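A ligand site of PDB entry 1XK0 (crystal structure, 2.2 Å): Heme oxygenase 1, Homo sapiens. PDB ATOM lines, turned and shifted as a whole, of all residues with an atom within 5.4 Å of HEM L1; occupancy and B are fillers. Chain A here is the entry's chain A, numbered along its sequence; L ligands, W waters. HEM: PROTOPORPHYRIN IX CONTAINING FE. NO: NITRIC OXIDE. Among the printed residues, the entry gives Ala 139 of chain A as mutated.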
ATOM      1  N   SER A  14       9.635  23.007  -1.320  1.00  0.00           N
ATOM      2  CA  SER A  14       8.527  22.293  -1.959  1.00  0.00           C
ATOM      3  C   SER A  14       7.989  23.118  -3.122  1.00  0.00           C
ATOM      4  O   SER A  14       7.639  22.568  -4.171  1.00  0.00           O
ATOM      5  CB  SER A  14       7.405  22.060  -0.942  1.00  0.00           C
ATOM      6  OG  SER A  14       6.964  23.292  -0.401  1.00  0.00           O
ATOM      7  N   LEU A  17      10.730  23.319  -5.971  1.00  0.00           N
ATOM      8  CA  LEU A  17      10.801  22.066  -6.726  1.00  0.00           C
ATOM      9  C   LEU A  17       9.691  21.950  -7.773  1.00  0.00           C
ATOM     10  O   LEU A  17       9.933  21.489  -8.891  1.00  0.00           O
ATOM     11  CB  LEU A  17      10.741  20.865  -5.780  1.00  0.00           C
ATOM     12  CG  LEU A  17      12.044  20.495  -5.077  1.00  0.00           C
ATOM     13  CD1 LEU A  17      11.762  19.546  -3.932  1.00  0.00           C
ATOM     14  CD2 LEU A  17      12.985  19.866  -6.078  1.00  0.00           C
ATOM     15  N   LYS A  18       8.477  22.355  -7.421  1.00  0.00           N
ATOM     16  CA  LYS A  18       7.358  22.263  -8.362  1.00  0.00           C
ATOM     17  C   LYS A  18       7.606  23.117  -9.598  1.00  0.00           C
ATOM     18  O   LYS A  18       7.482  22.655 -10.724  1.00  0.00           O
ATOM     19  CB  LYS A  18       6.054  22.672  -7.683  1.00  0.00           C
ATOM     20  CG  LYS A  18       4.811  22.217  -8.415  1.00  0.00           C
ATOM     21  CD  LYS A  18       3.556  22.543  -7.634  1.00  0.00           C
ATOM     22  CE  LYS A  18       2.326  21.941  -8.295  1.00  0.00           C
ATOM     23  NZ  LYS A  18       1.049  22.280  -7.585  1.00  0.00           N
ATOM     24  N   HIS A  25       8.656  17.614 -16.144  1.00  0.00           N
ATOM     25  CA  HIS A  25       7.405  16.929 -15.847  1.00  0.00           C
ATOM     26  C   HIS A  25       6.576  16.819 -17.121  1.00  0.00           C
ATOM     27  O   HIS A  25       5.978  15.777 -17.397  1.00  0.00           O
ATOM     28  CB  HIS A  25       6.620  17.677 -14.778  1.00  0.00           C
ATOM     29  CG  HIS A  25       5.377  16.972 -14.329  1.00  0.00           C
ATOM     30  ND1 HIS A  25       4.296  16.755 -15.158  1.00  0.00           N
ATOM     31  CD2 HIS A  25       5.038  16.415 -13.144  1.00  0.00           C
ATOM     32  CE1 HIS A  25       3.349  16.101 -14.507  1.00  0.00           C
ATOM     33  NE2 HIS A  25       3.776  15.883 -13.275  1.00  0.00           N
ATOM     34  N   ALA A  28       8.202  14.318 -19.264  1.00  0.00           N
ATOM     35  CA  ALA A  28       7.860  12.989 -18.781  1.00  0.00           C
ATOM     36  C   ALA A  28       6.490  12.630 -19.332  1.00  0.00           C
ATOM     37  O   ALA A  28       6.264  11.512 -19.790  1.00  0.00           O
ATOM     38  CB  ALA A  28       7.829  12.970 -17.260  1.00  0.00           C
ATOM     39  N   GLU A  29       5.584  13.596 -19.290  1.00  0.00           N
ATOM     40  CA  GLU A  29       4.233  13.400 -19.797  1.00  0.00           C
ATOM     41  C   GLU A  29       4.251  13.016 -21.271  1.00  0.00           C
ATOM     42  O   GLU A  29       3.552  12.080 -21.668  1.00  0.00           O
ATOM     43  CB  GLU A  29       3.400  14.661 -19.623  1.00  0.00           C
ATOM     44  CG  GLU A  29       3.026  14.959 -18.188  1.00  0.00           C
ATOM     45  CD  GLU A  29       2.045  16.104 -18.078  1.00  0.00           C
ATOM     46  OE1 GLU A  29       0.922  15.978 -18.619  1.00  0.00           O
ATOM     47  OE2 GLU A  29       2.406  17.128 -17.460  1.00  0.00           O
ATOM     48  N   MET A  34       4.466   6.719 -21.567  1.00  0.00           N
ATOM     49  CA  MET A  34       3.654   7.378 -20.545  1.00  0.00           C
ATOM     50  C   MET A  34       2.381   8.012 -21.109  1.00  0.00           C
ATOM     51  O   MET A  34       1.315   7.897 -20.513  1.00  0.00           O
ATOM     52  CB  MET A  34       4.482   8.432 -19.818  1.00  0.00           C
ATOM     53  CG  MET A  34       3.775   9.077 -18.634  1.00  0.00           C
ATOM     54  SD  MET A  34       3.168   7.901 -17.394  1.00  0.00           S
ATOM     55  CE  MET A  34       4.513   6.738 -17.328  1.00  0.00           C
ATOM     56  N   ARG A  35       2.499   8.693 -22.243  1.00  0.00           N
ATOM     57  CA  ARG A  35       1.331   9.322 -22.837  1.00  0.00           C
ATOM     58  C   ARG A  35       0.355   8.232 -23.279  1.00  0.00           C
ATOM     59  O   ARG A  35      -0.857   8.366 -23.105  1.00  0.00           O
ATOM     60  CB  ARG A  35       1.744  10.190 -24.033  1.00  0.00           C
ATOM     61  CG  ARG A  35       2.410   9.430 -25.170  1.00  0.00           C
ATOM     62  CD  ARG A  35       2.971  10.372 -26.234  1.00  0.00           C
ATOM     63  NE  ARG A  35       3.446   9.629 -27.396  1.00  0.00           N
ATOM     64  CZ  ARG A  35       4.096  10.162 -28.420  1.00  0.00           C
ATOM     65  NH1 ARG A  35       4.361  11.456 -28.419  1.00  0.00           N
ATOM     66  NH2 ARG A  35       4.483   9.405 -29.432  1.00  0.00           N
ATOM     67  N   GLN A  38      -1.304   7.008 -20.361  1.00  0.00           N
ATOM     68  CA  GLN A  38      -2.231   8.086 -20.018  1.00  0.00           C
ATOM     69  C   GLN A  38      -3.521   8.002 -20.839  1.00  0.00           C
ATOM     70  O   GLN A  38      -4.562   8.463 -20.396  1.00  0.00           O
ATOM     71  CB  GLN A  38      -1.580   9.445 -20.246  1.00  0.00           C
ATOM     72  CG  GLN A  38      -2.506  10.627 -20.071  1.00  0.00           C
ATOM     73  CD  GLN A  38      -1.873  11.955 -20.438  1.00  0.00           C
ATOM     74  OE1 GLN A  38      -2.515  13.008 -20.379  1.00  0.00           O
ATOM     75  NE2 GLN A  38      -0.595  11.929 -20.819  1.00  0.00           N
ATOM     76  N   TYR A 134      11.218  12.605  -3.159  1.00  0.00           N
ATOM     77  CA  TYR A 134      10.165  13.537  -3.538  1.00  0.00           C
ATOM     78  C   TYR A 134       9.613  13.216  -4.934  1.00  0.00           C
ATOM     79  O   TYR A 134       8.401  13.175  -5.134  1.00  0.00           O
ATOM     80  CB  TYR A 134      10.706  14.966  -3.516  1.00  0.00           C
ATOM     81  CG  TYR A 134       9.946  15.944  -4.389  1.00  0.00           C
ATOM     82  CD1 TYR A 134       8.794  16.582  -3.918  1.00  0.00           C
ATOM     83  CD2 TYR A 134      10.381  16.228  -5.677  1.00  0.00           C
ATOM     84  CE1 TYR A 134       8.084  17.475  -4.725  1.00  0.00           C
ATOM     85  CE2 TYR A 134       9.684  17.119  -6.500  1.00  0.00           C
ATOM     86  CZ  TYR A 134       8.530  17.740  -6.015  1.00  0.00           C
ATOM     87  OH  TYR A 134       7.839  18.618  -6.818  1.00  0.00           O
ATOM     88  N   THR A 135      10.501  12.993  -5.893  1.00  0.00           N
ATOM     89  CA  THR A 135      10.086  12.707  -7.263  1.00  0.00           C
ATOM     90  C   THR A 135       9.245  11.424  -7.325  1.00  0.00           C
ATOM     91  O   THR A 135       8.149  11.412  -7.874  1.00  0.00           O
ATOM     92  CB  THR A 135      11.313  12.558  -8.169  1.00  0.00           C
ATOM     93  OG1 THR A 135      12.100  13.753  -8.098  1.00  0.00           O
ATOM     94  CG2 THR A 135      10.889  12.319  -9.616  1.00  0.00           C
ATOM     95  N   ARG A 136       9.787  10.359  -6.755  1.00  0.00           N
ATOM     96  CA  ARG A 136       9.124   9.069  -6.727  1.00  0.00           C
ATOM     97  C   ARG A 136       7.838   9.040  -5.907  1.00  0.00           C
ATOM     98  O   ARG A 136       6.745   8.802  -6.446  1.00  0.00           O
ATOM     99  CB  ARG A 136      10.088   8.009  -6.208  1.00  0.00           C
ATOM    100  CG  ARG A 136      10.801   7.220  -7.277  1.00  0.00           C
ATOM    101  CD  ARG A 136      10.045   5.945  -7.632  1.00  0.00           C
ATOM    102  NE  ARG A 136       8.818   6.167  -8.408  1.00  0.00           N
ATOM    103  CZ  ARG A 136       8.799   6.496  -9.692  1.00  0.00           C
ATOM    104  NH1 ARG A 136       9.938   6.662 -10.352  1.00  0.00           N
ATOM    105  NH2 ARG A 136       7.642   6.630 -10.336  1.00  0.00           N
ATOM    106  N   LEU A 138       5.911  11.407  -4.382  1.00  0.00           N
ATOM    107  CA  LEU A 138       4.834  12.305  -4.776  1.00  0.00           C
ATOM    108  C   LEU A 138       4.292  11.979  -6.163  1.00  0.00           C
ATOM    109  O   LEU A 138       3.160  12.328  -6.496  1.00  0.00           O
ATOM    110  CB  LEU A 138       5.293  13.756  -4.693  1.00  0.00           C
ATOM    111  CG  LEU A 138       4.965  14.378  -3.333  1.00  0.00           C
ATOM    112  CD1 LEU A 138       5.552  13.527  -2.218  1.00  0.00           C
ATOM    113  CD2 LEU A 138       5.494  15.797  -3.268  1.00  0.00           C
ATOM    114  N   ALA A 139       5.104  11.316  -6.979  1.00  0.00           N
ATOM    115  CA  ALA A 139       4.681  10.920  -8.313  1.00  0.00           C
ATOM    116  C   ALA A 139       3.689   9.774  -8.155  1.00  0.00           C
ATOM    117  O   ALA A 139       2.581   9.814  -8.669  1.00  0.00           O
ATOM    118  CB  ALA A 139       5.860  10.461  -9.136  1.00  0.00           C
ATOM    119  N   SER A 142       0.556  10.931  -6.184  1.00  0.00           N
ATOM    120  CA  SER A 142      -0.327  11.840  -6.912  1.00  0.00           C
ATOM    121  C   SER A 142      -1.085  11.217  -8.082  1.00  0.00           C
ATOM    122  O   SER A 142      -2.296  11.290  -8.144  1.00  0.00           O
ATOM    123  CB  SER A 142       0.476  13.041  -7.422  1.00  0.00           C
ATOM    124  OG  SER A 142       0.976  13.818  -6.337  1.00  0.00           O
ATOM    125  N   LYS A 179       0.596  14.830   1.690  1.00  0.00           N
ATOM    126  CA  LYS A 179       1.407  15.675   0.813  1.00  0.00           C
ATOM    127  C   LYS A 179       1.764  16.983   1.529  1.00  0.00           C
ATOM    128  O   LYS A 179       2.921  17.428   1.460  1.00  0.00           O
ATOM    129  CB  LYS A 179       0.662  15.945  -0.499  1.00  0.00           C
ATOM    130  CG  LYS A 179       0.821  14.800  -1.509  1.00  0.00           C
ATOM    131  CD  LYS A 179      -0.401  14.609  -2.440  1.00  0.00           C
ATOM    132  CE  LYS A 179      -0.587  15.746  -3.444  1.00  0.00           C
ATOM    133  NZ  LYS A 179      -0.995  17.030  -2.782  1.00  0.00           N
ATOM    134  N   GLU A 183       5.502  18.008   2.287  1.00  0.00           N
ATOM    135  CA  GLU A 183       6.071  19.251   1.792  1.00  0.00           C
ATOM    136  C   GLU A 183       6.626  20.052   2.968  1.00  0.00           C
ATOM    137  O   GLU A 183       7.717  20.626   2.880  1.00  0.00           O
ATOM    138  CB  GLU A 183       5.006  20.054   1.023  1.00  0.00           C
ATOM    139  CG  GLU A 183       4.587  19.374  -0.281  1.00  0.00           C
ATOM    140  CD  GLU A 183       3.547  20.173  -1.081  1.00  0.00           C
ATOM    141  OE1 GLU A 183       3.735  21.397  -1.221  1.00  0.00           O
ATOM    142  OE2 GLU A 183       2.562  19.586  -1.575  1.00  0.00           O
ATOM    143  N   PHE A 207      13.549  13.023 -12.898  1.00  0.00           N
ATOM    144  CA  PHE A 207      12.554  12.929 -13.972  1.00  0.00           C
ATOM    145  C   PHE A 207      13.208  12.376 -15.224  1.00  0.00           C
ATOM    146  O   PHE A 207      12.647  11.501 -15.893  1.00  0.00           O
ATOM    147  CB  PHE A 207      11.934  14.285 -14.310  1.00  0.00           C
ATOM    148  CG  PHE A 207      10.861  14.714 -13.373  1.00  0.00           C
ATOM    149  CD1 PHE A 207      11.167  15.330 -12.163  1.00  0.00           C
ATOM    150  CD2 PHE A 207       9.521  14.506 -13.703  1.00  0.00           C
ATOM    151  CE1 PHE A 207      10.164  15.752 -11.299  1.00  0.00           C
ATOM    152  CE2 PHE A 207       8.505  14.912 -12.846  1.00  0.00           C
ATOM    153  CZ  PHE A 207       8.822  15.540 -11.641  1.00  0.00           C
ATOM    154  N   ASN A 210      13.541   8.791 -15.259  1.00  0.00           N
ATOM    155  CA  ASN A 210      12.263   8.143 -15.489  1.00  0.00           C
ATOM    156  C   ASN A 210      11.970   8.212 -16.967  1.00  0.00           C
ATOM    157  O   ASN A 210      11.643   7.198 -17.584  1.00  0.00           O
ATOM    158  CB  ASN A 210      11.160   8.854 -14.693  1.00  0.00           C
ATOM    159  CG  ASN A 210      11.111   8.387 -13.252  1.00  0.00           C
ATOM    160  OD1 ASN A 210      10.566   7.321 -12.955  1.00  0.00           O
ATOM    161  ND2 ASN A 210      11.695   9.162 -12.357  1.00  0.00           N
ATOM    162  N   PHE A 214      11.073   5.221 -19.544  1.00  0.00           N
ATOM    163  CA  PHE A 214       9.927   5.054 -20.431  1.00  0.00           C
ATOM    164  C   PHE A 214      10.408   4.826 -21.842  1.00  0.00           C
ATOM    165  O   PHE A 214      10.017   3.849 -22.490  1.00  0.00           O
ATOM    166  CB  PHE A 214       9.018   6.277 -20.403  1.00  0.00           C
ATOM    167  CG  PHE A 214       8.500   6.606 -19.049  1.00  0.00           C
ATOM    168  CD1 PHE A 214       8.111   5.584 -18.185  1.00  0.00           C
ATOM    169  CD2 PHE A 214       8.385   7.924 -18.633  1.00  0.00           C
ATOM    170  CE1 PHE A 214       7.618   5.887 -16.923  1.00  0.00           C
ATOM    171  CE2 PHE A 214       7.899   8.226 -17.379  1.00  0.00           C
ATOM    172  CZ  PHE A 214       7.510   7.205 -16.514  1.00  0.00           C
HETATM  173  CHA HEM L   1       2.183  16.066  -9.605  1.00  0.00           C
HETATM  174  CHB HEM L   1      -0.011  14.736 -13.784  1.00  0.00           C
HETATM  175  CHC HEM L   1       3.738  11.836 -14.838  1.00  0.00           C
HETATM  176  CHD HEM L   1       6.005  13.375 -10.836  1.00  0.00           C
HETATM  177  C1A HEM L   1       1.255  15.937 -10.673  1.00  0.00           C
HETATM  178  C2A HEM L   1      -0.018  16.633 -10.781  1.00  0.00           C
HETATM  179  C3A HEM L   1      -0.540  16.394 -11.999  1.00  0.00           C
HETATM  180  C4A HEM L   1       0.339  15.426 -12.614  1.00  0.00           C
HETATM  181  CMA HEM L   1      -1.719  17.099 -12.651  1.00  0.00           C
HETATM  182  CAA HEM L   1      -0.749  17.368  -9.667  1.00  0.00           C
HETATM  183  CBA HEM L   1      -0.146  18.734  -9.407  1.00  0.00           C
HETATM  184  CGA HEM L   1      -0.107  19.056  -7.931  1.00  0.00           C
HETATM  185  O1A HEM L   1      -1.199  19.099  -7.301  1.00  0.00           O
HETATM  186  O2A HEM L   1       1.005  19.265  -7.397  1.00  0.00           O
HETATM  187  C1B HEM L   1       0.794  13.787 -14.384  1.00  0.00           C
HETATM  188  C2B HEM L   1       0.499  13.214 -15.695  1.00  0.00           C
HETATM  189  C3B HEM L   1       1.558  12.379 -16.007  1.00  0.00           C
HETATM  190  C4B HEM L   1       2.522  12.510 -14.898  1.00  0.00           C
HETATM  191  CMB HEM L   1      -0.686  13.606 -16.578  1.00  0.00           C
HETATM  192  CAB HEM L   1       1.699  11.520 -17.123  1.00  0.00           C
HETATM  193  CBB HEM L   1       1.102  11.690 -18.457  1.00  0.00           C
HETATM  194  C1C HEM L   1       4.658  12.001 -13.821  1.00  0.00           C
HETATM  195  C2C HEM L   1       5.941  11.304 -13.782  1.00  0.00           C
HETATM  196  C3C HEM L   1       6.596  11.739 -12.666  1.00  0.00           C
HETATM  197  C4C HEM L   1       5.698  12.698 -12.000  1.00  0.00           C
HETATM  198  CMC HEM L   1       6.511  10.349 -14.812  1.00  0.00           C
HETATM  199  CAC HEM L   1       7.900  11.408 -12.289  1.00  0.00           C
HETATM  200  CBC HEM L   1       8.471  10.080 -12.237  1.00  0.00           C
HETATM  201  C1D HEM L   1       5.210  14.338 -10.204  1.00  0.00           C
HETATM  202  C2D HEM L   1       5.559  14.973  -8.975  1.00  0.00           C
HETATM  203  C3D HEM L   1       4.497  15.718  -8.576  1.00  0.00           C
HETATM  204  C4D HEM L   1       3.468  15.512  -9.597  1.00  0.00           C
HETATM  205  CMD HEM L   1       6.912  14.854  -8.280  1.00  0.00           C
HETATM  206  CAD HEM L   1       4.499  16.650  -7.357  1.00  0.00           C
HETATM  207  CBD HEM L   1       4.325  18.123  -7.730  1.00  0.00           C
HETATM  208  CGD HEM L   1       4.473  19.059  -6.550  1.00  0.00           C
HETATM  209  O1D HEM L   1       5.618  19.378  -6.160  1.00  0.00           O
HETATM  210  O2D HEM L   1       3.427  19.489  -6.003  1.00  0.00           O
HETATM  211  NA  HEM L   1       1.472  15.202 -11.835  1.00  0.00           N
HETATM  212  NB  HEM L   1       2.060  13.401 -13.914  1.00  0.00           N
HETATM  213  NC  HEM L   1       4.506  12.860 -12.727  1.00  0.00           N
HETATM  214  ND  HEM L   1       3.953  14.689 -10.624  1.00  0.00           N
HETATM  215 FE   HEM L   1       3.031  14.120 -12.292  1.00  0.00          FE
HETATM  216  N    NO L   2       2.220  12.799 -11.091  1.00  0.00           N
HETATM  217  O    NO L   2       1.631  11.801 -11.096  1.00  0.00           O
HETATM  218  O   HOH W   1      -0.241   9.936 -14.429  1.00  0.00           O
HETATM  219  O   HOH W   2       5.583  20.834  -4.081  1.00  0.00           O
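OH of Tyr 134 lies within hydrogen-bond range of O1D of HEM L1.
NE2 of His 25 is bound to FE of HEM L1, at 2.2 Å.
The side-chain amino group of Lys 18 lies within salt-bridge range of an oxygen (O2A) of HEM L1 (3.0 Å).
An iron atom (FE) of HEM L1 is bound by a nitrogen (N) of NO L2 (2.0 Å).
A ring nitrogen (ND1) of His 25 is in hydrogen-bond range of the side-chain carboxylate of Glu 29 (3.0 Å).
The guanidinium group (NH1) of Arg 136 sits at hydrogen-bond distance from the side-chain amide oxygen (OD1) of Asn 210 (2.8 Å).
Ala 28 touches HEM L1.
Glu 29 touches HEM L1.
Met 34 touches HEM L1 (CG to CAB, 3.5 Å).
Gln 38 touches HEM L1 (NE2 to CBB, 2.9 Å).
Thr 135 touches HEM L1.
Ala 139 touches HEM L1 (CB to CHD, 3.4 Å).
Phe 207 touches HEM L1.
CG of Asn 210 touches CBC of HEM L1, 3.3 Å away.
Phe 214 touches HEM L1.
Hydrophobic or aromatic side chains that line HEM L1: His 25, Ala 28, Met 34, Tyr 134, Ala 139, Phe 207 and Phe 214.
12 residues have an atom within 4 Å of HEM L1: Lys 18, His 25, Ala 28, Glu 29, Met 34, Gln 38, Tyr 134, Thr 135, Ala 139, Phe 207, Asn 210 and Phe 214.
Water W2 lies within hydrogen-bond range of O1D of HEM L1, O of Ser 14 and OE1 of Glu 183.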
